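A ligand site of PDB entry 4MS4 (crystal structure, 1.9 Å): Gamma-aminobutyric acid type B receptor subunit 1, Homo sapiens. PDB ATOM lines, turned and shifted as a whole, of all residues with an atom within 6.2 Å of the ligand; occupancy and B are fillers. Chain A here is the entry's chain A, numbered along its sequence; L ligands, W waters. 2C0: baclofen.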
ATOM      1  N   GLY A  17      -8.829 -16.144 -23.090  1.00  0.00           N
ATOM      2  CA  GLY A  17      -8.921 -17.235 -24.072  1.00  0.00           C
ATOM      3  C   GLY A  17      -9.649 -16.859 -25.361  1.00  0.00           C
ATOM      4  O   GLY A  17      -9.080 -16.917 -26.443  1.00  0.00           O
ATOM      5  N   TRP A  18     -10.886 -16.434 -25.212  1.00  0.00           N
ATOM      6  CA  TRP A  18     -11.729 -15.961 -26.309  1.00  0.00           C
ATOM      7  C   TRP A  18     -12.247 -14.576 -25.917  1.00  0.00           C
ATOM      8  O   TRP A  18     -13.159 -14.491 -25.090  1.00  0.00           O
ATOM      9  CB  TRP A  18     -12.902 -16.909 -26.537  1.00  0.00           C
ATOM     10  CG  TRP A  18     -13.870 -16.423 -27.579  1.00  0.00           C
ATOM     11  CD1 TRP A  18     -13.609 -16.193 -28.900  1.00  0.00           C
ATOM     12  CD2 TRP A  18     -15.246 -16.116 -27.380  1.00  0.00           C
ATOM     13  NE1 TRP A  18     -14.744 -15.782 -29.539  1.00  0.00           N
ATOM     14  CE2 TRP A  18     -15.768 -15.723 -28.640  1.00  0.00           C
ATOM     15  CE3 TRP A  18     -16.109 -16.143 -26.263  1.00  0.00           C
ATOM     16  CZ2 TRP A  18     -17.120 -15.399 -28.815  1.00  0.00           C
ATOM     17  CZ3 TRP A  18     -17.446 -15.827 -26.452  1.00  0.00           C
ATOM     18  CH2 TRP A  18     -17.941 -15.468 -27.711  1.00  0.00           C
ATOM     19  N   CYS A  56     -12.698 -13.869 -19.666  1.00  0.00           N
ATOM     20  CA  CYS A  56     -12.694 -15.302 -20.014  1.00  0.00           C
ATOM     21  C   CYS A  56     -11.961 -16.087 -18.891  1.00  0.00           C
ATOM     22  O   CYS A  56     -11.167 -17.006 -19.141  1.00  0.00           O
ATOM     23  CB  CYS A  56     -12.021 -15.482 -21.374  1.00  0.00           C
ATOM     24  SG  CYS A  56     -12.451 -17.025 -22.204  1.00  0.00           S
ATOM     25  N   GLY A  81     -20.398 -16.004 -21.463  1.00  0.00           N
ATOM     26  CA  GLY A  81     -19.814 -16.174 -22.792  1.00  0.00           C
ATOM     27  C   GLY A  81     -18.976 -17.415 -22.994  1.00  0.00           C
ATOM     28  O   GLY A  81     -19.452 -18.371 -23.615  1.00  0.00           O
ATOM     29  N   CYS A  82     -17.724 -17.395 -22.520  1.00  0.00           N
ATOM     30  CA  CYS A  82     -16.670 -18.445 -22.610  1.00  0.00           C
ATOM     31  C   CYS A  82     -17.184 -19.782 -22.058  1.00  0.00           C
ATOM     32  O   CYS A  82     -17.977 -19.794 -21.133  1.00  0.00           O
ATOM     33  CB  CYS A  82     -15.396 -17.998 -21.867  1.00  0.00           C
ATOM     34  SG  CYS A  82     -14.394 -16.781 -22.780  1.00  0.00           S
ATOM     35  N   SER A  83     -16.615 -20.898 -22.548  1.00  0.00           N
ATOM     36  CA  SER A  83     -16.952 -22.232 -22.053  1.00  0.00           C
ATOM     37  C   SER A  83     -16.618 -22.401 -20.561  1.00  0.00           C
ATOM     38  O   SER A  83     -17.449 -22.939 -19.827  1.00  0.00           O
ATOM     39  CB  SER A  83     -16.212 -23.316 -22.837  1.00  0.00           C
ATOM     40  OG  SER A  83     -16.894 -23.489 -24.073  1.00  0.00           O
ATOM     41  N   SER A  84     -15.420 -21.944 -20.112  1.00  0.00           N
ATOM     42  CA  SER A  84     -15.009 -22.135 -18.711  1.00  0.00           C
ATOM     43  C   SER A  84     -15.933 -21.363 -17.755  1.00  0.00           C
ATOM     44  O   SER A  84     -16.313 -21.880 -16.706  1.00  0.00           O
ATOM     45  CB  SER A  84     -13.546 -21.771 -18.496  1.00  0.00           C
ATOM     46  OG  SER A  84     -13.370 -20.361 -18.584  1.00  0.00           O
ATOM     47  N   GLY A 104     -21.887 -17.856 -26.344  1.00  0.00           N
ATOM     48  CA  GLY A 104     -20.579 -18.188 -26.862  1.00  0.00           C
ATOM     49  C   GLY A 104     -19.956 -19.526 -26.537  1.00  0.00           C
ATOM     50  O   GLY A 104     -18.907 -19.844 -27.100  1.00  0.00           O
ATOM     51  N   SER A 105     -20.529 -20.306 -25.608  1.00  0.00           N
ATOM     52  CA  SER A 105     -19.919 -21.539 -25.113  1.00  0.00           C
ATOM     53  C   SER A 105     -20.054 -22.754 -26.040  1.00  0.00           C
ATOM     54  O   SER A 105     -21.158 -23.277 -26.192  1.00  0.00           O
ATOM     55  CB  SER A 105     -20.473 -21.877 -23.733  1.00  0.00           C
ATOM     56  OG  SER A 105     -21.829 -22.255 -23.872  1.00  0.00           O
ATOM     57  N   SER A 106     -18.945 -23.266 -26.538  1.00  0.00           N
ATOM     58  CA  SER A 106     -18.945 -24.411 -27.443  1.00  0.00           C
ATOM     59  C   SER A 106     -18.711 -25.764 -26.731  1.00  0.00           C
ATOM     60  O   SER A 106     -18.819 -26.794 -27.382  1.00  0.00           O
ATOM     61  CB  SER A 106     -17.869 -24.217 -28.496  1.00  0.00           C
ATOM     62  OG  SER A 106     -16.607 -24.346 -27.873  1.00  0.00           O
ATOM     63  N   SER A 107     -18.374 -25.756 -25.429  1.00  0.00           N
ATOM     64  CA  SER A 107     -18.034 -26.993 -24.729  1.00  0.00           C
ATOM     65  C   SER A 107     -19.056 -28.104 -24.928  1.00  0.00           C
ATOM     66  O   SER A 107     -20.178 -27.961 -24.470  1.00  0.00           O
ATOM     67  CB  SER A 107     -17.743 -26.782 -23.234  1.00  0.00           C
ATOM     68  OG  SER A 107     -17.386 -28.035 -22.654  1.00  0.00           O
ATOM     69  N   HIS A 123     -24.899 -20.913 -29.186  1.00  0.00           N
ATOM     70  CA  HIS A 123     -23.674 -21.352 -29.828  1.00  0.00           C
ATOM     71  C   HIS A 123     -23.754 -22.865 -30.049  1.00  0.00           C
ATOM     72  O   HIS A 123     -24.133 -23.581 -29.129  1.00  0.00           O
ATOM     73  CB  HIS A 123     -22.423 -21.016 -28.965  1.00  0.00           C
ATOM     74  CG  HIS A 123     -21.114 -21.126 -29.721  1.00  0.00           C
ATOM     75  ND1 HIS A 123     -20.622 -22.345 -30.142  1.00  0.00           N
ATOM     76  CD2 HIS A 123     -20.215 -20.163 -30.035  1.00  0.00           C
ATOM     77  CE1 HIS A 123     -19.478 -22.097 -30.751  1.00  0.00           C
ATOM     78  NE2 HIS A 123     -19.168 -20.798 -30.674  1.00  0.00           N
ATOM     79  N   VAL A 154     -13.689 -27.783 -22.490  1.00  0.00           N
ATOM     80  CA  VAL A 154     -14.158 -27.541 -23.865  1.00  0.00           C
ATOM     81  C   VAL A 154     -13.386 -28.444 -24.890  1.00  0.00           C
ATOM     82  O   VAL A 154     -13.992 -29.083 -25.740  1.00  0.00           O
ATOM     83  CB  VAL A 154     -14.135 -26.016 -24.255  1.00  0.00           C
ATOM     84  CG1 VAL A 154     -12.798 -25.376 -23.915  1.00  0.00           C
ATOM     85  CG2 VAL A 154     -14.474 -25.805 -25.728  1.00  0.00           C
ATOM     86  N   PHE A 155     -12.061 -28.489 -24.761  1.00  0.00           N
ATOM     87  CA  PHE A 155     -11.191 -29.235 -25.653  1.00  0.00           C
ATOM     88  C   PHE A 155     -11.193 -30.713 -25.339  1.00  0.00           C
ATOM     89  O   PHE A 155     -11.307 -31.514 -26.255  1.00  0.00           O
ATOM     90  CB  PHE A 155      -9.755 -28.659 -25.642  1.00  0.00           C
ATOM     91  CG  PHE A 155      -9.744 -27.168 -25.910  1.00  0.00           C
ATOM     92  CD1 PHE A 155     -10.382 -26.633 -27.026  1.00  0.00           C
ATOM     93  CD2 PHE A 155      -9.168 -26.285 -24.995  1.00  0.00           C
ATOM     94  CE1 PHE A 155     -10.422 -25.245 -27.240  1.00  0.00           C
ATOM     95  CE2 PHE A 155      -9.218 -24.895 -25.198  1.00  0.00           C
ATOM     96  CZ  PHE A 155      -9.833 -24.390 -26.327  1.00  0.00           C
ATOM     97  N   LEU A 201      -6.109 -28.722 -30.263  1.00  0.00           N
ATOM     98  CA  LEU A 201      -7.263 -28.014 -29.679  1.00  0.00           C
ATOM     99  C   LEU A 201      -6.848 -27.132 -28.524  1.00  0.00           C
ATOM    100  O   LEU A 201      -6.441 -27.655 -27.484  1.00  0.00           O
ATOM    101  CB  LEU A 201      -8.364 -29.000 -29.210  1.00  0.00           C
ATOM    102  CG  LEU A 201      -8.750 -30.102 -30.237  1.00  0.00           C
ATOM    103  CD1 LEU A 201      -9.718 -31.087 -29.621  1.00  0.00           C
ATOM    104  CD2 LEU A 201      -9.351 -29.478 -31.527  1.00  0.00           C
ATOM    105  N   PHE A 202      -6.900 -25.796 -28.732  1.00  0.00           N
ATOM    106  CA  PHE A 202      -6.484 -24.811 -27.718  1.00  0.00           C
ATOM    107  C   PHE A 202      -6.942 -23.433 -28.117  1.00  0.00           C
ATOM    108  O   PHE A 202      -7.231 -23.189 -29.288  1.00  0.00           O
ATOM    109  CB  PHE A 202      -4.947 -24.798 -27.491  1.00  0.00           C
ATOM    110  CG  PHE A 202      -4.132 -25.278 -28.672  1.00  0.00           C
ATOM    111  CD1 PHE A 202      -3.947 -24.468 -29.792  1.00  0.00           C
ATOM    112  CD2 PHE A 202      -3.602 -26.566 -28.701  1.00  0.00           C
ATOM    113  CE1 PHE A 202      -3.238 -24.939 -30.908  1.00  0.00           C
ATOM    114  CE2 PHE A 202      -2.923 -27.033 -29.816  1.00  0.00           C
ATOM    115  CZ  PHE A 202      -2.740 -26.219 -30.920  1.00  0.00           C
ATOM    116  N   TYR A 203      -6.947 -22.493 -27.147  1.00  0.00           N
ATOM    117  CA  TYR A 203      -7.296 -21.100 -27.472  1.00  0.00           C
ATOM    118  C   TYR A 203      -6.116 -20.450 -28.173  1.00  0.00           C
ATOM    119  O   TYR A 203      -5.003 -20.983 -28.140  1.00  0.00           O
ATOM    120  CB  TYR A 203      -7.667 -20.308 -26.204  1.00  0.00           C
ATOM    121  CG  TYR A 203      -9.037 -20.675 -25.666  1.00  0.00           C
ATOM    122  CD1 TYR A 203     -10.197 -20.396 -26.390  1.00  0.00           C
ATOM    123  CD2 TYR A 203      -9.170 -21.295 -24.423  1.00  0.00           C
ATOM    124  CE1 TYR A 203     -11.454 -20.713 -25.890  1.00  0.00           C
ATOM    125  CE2 TYR A 203     -10.413 -21.640 -23.926  1.00  0.00           C
ATOM    126  CZ  TYR A 203     -11.547 -21.361 -24.663  1.00  0.00           C
ATOM    127  OH  TYR A 203     -12.765 -21.691 -24.123  1.00  0.00           O
ATOM    128  N   GLU A 204      -6.358 -19.298 -28.805  1.00  0.00           N
ATOM    129  CA  GLU A 204      -5.352 -18.538 -29.551  1.00  0.00           C
ATOM    130  C   GLU A 204      -4.079 -18.300 -28.761  1.00  0.00           C
ATOM    131  O   GLU A 204      -3.009 -18.485 -29.313  1.00  0.00           O
ATOM    132  CB  GLU A 204      -5.934 -17.204 -30.043  1.00  0.00           C
ATOM    133  CG  GLU A 204      -5.048 -16.476 -31.029  1.00  0.00           C
ATOM    134  CD  GLU A 204      -5.601 -15.129 -31.436  1.00  0.00           C
ATOM    135  OE1 GLU A 204      -6.792 -15.061 -31.815  1.00  0.00           O
ATOM    136  OE2 GLU A 204      -4.838 -14.135 -31.412  1.00  0.00           O
ATOM    137  N   ILE A 229      -8.661 -25.019 -34.678  1.00  0.00           N
ATOM    138  CA  ILE A 229      -9.974 -24.390 -34.582  1.00  0.00           C
ATOM    139  C   ILE A 229      -9.853 -23.004 -35.281  1.00  0.00           C
ATOM    140  O   ILE A 229      -8.873 -22.301 -35.057  1.00  0.00           O
ATOM    141  CB  ILE A 229     -10.360 -24.275 -33.074  1.00  0.00           C
ATOM    142  CG1 ILE A 229     -10.480 -25.701 -32.466  1.00  0.00           C
ATOM    143  CG2 ILE A 229     -11.693 -23.551 -32.921  1.00  0.00           C
ATOM    144  CD1 ILE A 229     -10.517 -25.710 -30.871  1.00  0.00           C
ATOM    145  N   TRP A 231     -11.340 -20.140 -34.927  1.00  0.00           N
ATOM    146  CA  TRP A 231     -11.872 -18.957 -34.243  1.00  0.00           C
ATOM    147  C   TRP A 231     -10.840 -17.872 -33.904  1.00  0.00           C
ATOM    148  O   TRP A 231     -11.201 -16.862 -33.317  1.00  0.00           O
ATOM    149  CB  TRP A 231     -12.652 -19.359 -32.974  1.00  0.00           C
ATOM    150  CG  TRP A 231     -13.878 -20.198 -33.209  1.00  0.00           C
ATOM    151  CD1 TRP A 231     -14.206 -21.352 -32.554  1.00  0.00           C
ATOM    152  CD2 TRP A 231     -14.963 -19.919 -34.108  1.00  0.00           C
ATOM    153  NE1 TRP A 231     -15.424 -21.807 -32.984  1.00  0.00           N
ATOM    154  CE2 TRP A 231     -15.918 -20.945 -33.937  1.00  0.00           C
ATOM    155  CE3 TRP A 231     -15.231 -18.887 -35.045  1.00  0.00           C
ATOM    156  CZ2 TRP A 231     -17.102 -21.010 -34.685  1.00  0.00           C
ATOM    157  CZ3 TRP A 231     -16.407 -18.938 -35.777  1.00  0.00           C
ATOM    158  CH2 TRP A 231     -17.345 -19.972 -35.590  1.00  0.00           C
ATOM    159  N   TYR A 232      -9.574 -18.053 -34.256  1.00  0.00           N
ATOM    160  CA  TYR A 232      -8.523 -17.105 -33.909  1.00  0.00           C
ATOM    161  C   TYR A 232      -8.588 -15.871 -34.817  1.00  0.00           C
ATOM    162  O   TYR A 232      -9.175 -15.928 -35.899  1.00  0.00           O
ATOM    163  CB  TYR A 232      -7.142 -17.737 -34.156  1.00  0.00           C
ATOM    164  CG  TYR A 232      -6.871 -19.083 -33.518  1.00  0.00           C
ATOM    165  CD1 TYR A 232      -7.575 -19.509 -32.399  1.00  0.00           C
ATOM    166  CD2 TYR A 232      -5.814 -19.875 -33.958  1.00  0.00           C
ATOM    167  CE1 TYR A 232      -7.314 -20.730 -31.789  1.00  0.00           C
ATOM    168  CE2 TYR A 232      -5.535 -21.109 -33.347  1.00  0.00           C
ATOM    169  CZ  TYR A 232      -6.264 -21.517 -32.255  1.00  0.00           C
ATOM    170  OH  TYR A 232      -5.989 -22.724 -31.652  1.00  0.00           O
ATOM    171  N   MET A 265     -22.137 -19.101 -38.784  1.00  0.00           N
ATOM    172  CA  MET A 265     -23.087 -18.587 -37.779  1.00  0.00           C
ATOM    173  C   MET A 265     -24.027 -17.520 -38.272  1.00  0.00           C
ATOM    174  O   MET A 265     -24.902 -17.114 -37.535  1.00  0.00           O
ATOM    175  CB  MET A 265     -22.315 -18.065 -36.564  1.00  0.00           C
ATOM    176  CG  MET A 265     -21.805 -19.177 -35.718  1.00  0.00           C
ATOM    177  SD  MET A 265     -20.511 -18.555 -34.656  1.00  0.00           S
ATOM    178  CE  MET A 265     -20.261 -20.047 -33.682  1.00  0.00           C
ATOM    179  N   GLU A 302     -19.121 -14.574 -33.804  1.00  0.00           N
ATOM    180  CA  GLU A 302     -20.124 -15.054 -32.829  1.00  0.00           C
ATOM    181  C   GLU A 302     -21.237 -14.052 -32.513  1.00  0.00           C
ATOM    182  O   GLU A 302     -22.273 -14.438 -31.977  1.00  0.00           O
ATOM    183  CB  GLU A 302     -19.460 -15.530 -31.519  1.00  0.00           C
ATOM    184  CG  GLU A 302     -18.511 -16.704 -31.702  1.00  0.00           C
ATOM    185  CD  GLU A 302     -17.088 -16.351 -32.107  1.00  0.00           C
ATOM    186  OE1 GLU A 302     -16.800 -15.156 -32.362  1.00  0.00           O
ATOM    187  OE2 GLU A 302     -16.249 -17.280 -32.154  1.00  0.00           O
HETATM  188 CL   2C0 L   1     -10.197 -22.178 -29.744  1.00  0.00          CL
HETATM  189  C8  2C0 L   1     -11.840 -21.590 -29.437  1.00  0.00           C
HETATM  190  C7  2C0 L   1     -12.087 -20.208 -29.327  1.00  0.00           C
HETATM  191  C6  2C0 L   1     -13.397 -19.788 -29.079  1.00  0.00           C
HETATM  192  C9  2C0 L   1     -12.844 -22.519 -29.239  1.00  0.00           C
HETATM  193  C10 2C0 L   1     -14.159 -22.107 -29.015  1.00  0.00           C
HETATM  194  C5  2C0 L   1     -14.432 -20.716 -28.941  1.00  0.00           C
HETATM  195  C2  2C0 L   1     -15.808 -20.299 -28.588  1.00  0.00           C
HETATM  196  C1  2C0 L   1     -16.313 -19.139 -29.476  1.00  0.00           C
HETATM  197  N   2C0 L   1     -16.537 -19.618 -30.849  1.00  0.00           N
HETATM  198  C3  2C0 L   1     -15.782 -19.806 -27.112  1.00  0.00           C
HETATM  199  C4  2C0 L   1     -15.705 -20.911 -26.073  1.00  0.00           C
HETATM  200  O2  2C0 L   1     -16.266 -22.004 -26.213  1.00  0.00           O
HETATM  201  O1  2C0 L   1     -15.052 -20.652 -24.936  1.00  0.00           O
HETATM  202  O   HOH W   1     -14.452 -25.315 -29.429  1.00  0.00           O
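The side-chain hydroxyl (OH) of Tyr 203 lies within hydrogen-bond range of an oxygen (O1) of the ligand, at 2.6 Å. The backbone NH (N) of Ser 83 is in hydrogen-bond range of an oxygen (O1) of the ligand. An oxygen (O2) of the ligand is in hydrogen-bond range of the side-chain hydroxyl (OG) of Ser 83 (2.7 Å). The side-chain carboxylate of Glu 302 is in salt-bridge range of a nitrogen (N) of the ligand (2.7 Å). A ring nitrogen (NE2) of His 123 is in hydrogen-bond range of a nitrogen (N) of the ligand (2.9 Å). The backbone NH of Ser 106 lies within hydrogen-bond range of an oxygen (O2) of the ligand, at 3.0 Å. The side-chain hydroxyl (OG) of Ser 106 sits at hydrogen-bond distance from an oxygen (O2) of the ligand (2.9 Å). The indole nitrogen of Trp 231 lies close to a nitrogen (N) of the ligand.
The side-chain hydroxyl (OG) of Ser 83 sits at hydrogen-bond distance from the backbone NH (N) of Ser 106. OG of Ser 83 sits at hydrogen-bond distance from N of Ser 107, at 3.0 Å. OE2 of Glu 302 lies within hydrogen-bond range of NE1 of Trp 18 (3.4 Å). O of Phe 202 is in hydrogen-bond range of OH of Tyr 232 (2.7 Å). The backbone NH (N) of Trp 18 is in hydrogen-bond range of the side-chain sulfur (SG) of Cys 56. The side-chain sulfur (SG) of Cys 82 forms a disulfide with the side-chain sulfur (SG) of Cys 56 (2.0 Å). The backbone NH (N) of Ser 105 is in hydrogen-bond range of the backbone carbonyl oxygen (O) of Gly 81, 3.0 Å away.
Merely in contact with the ligand: Gly 104 (3.1 Å), Phe 202 (3.2 Å), Trp 18 (3.6 Å), Cys 82 (3.6 Å), Ile 229 (3.7 Å), Tyr 232 (3.8 Å), Ser 105 (3.8 Å) and Phe 155 (3.97 Å). Hydrophobic or aromatic side chains that line the ligand: Trp 18, His 123, Phe 155, Tyr 203, Ile 229, Trp 231 and Tyr 232. Within 4 Å of the ligand: Trp 18, Cys 82, Ser 83, Gly 104, Ser 105, Ser 106, His 123, Phe 155, Phe 202, Tyr 203, Ile 229, Trp 231, Tyr 232 and Glu 302. The nearest printed residue that does not touch the ligand is Val 154 (4.2 Å).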
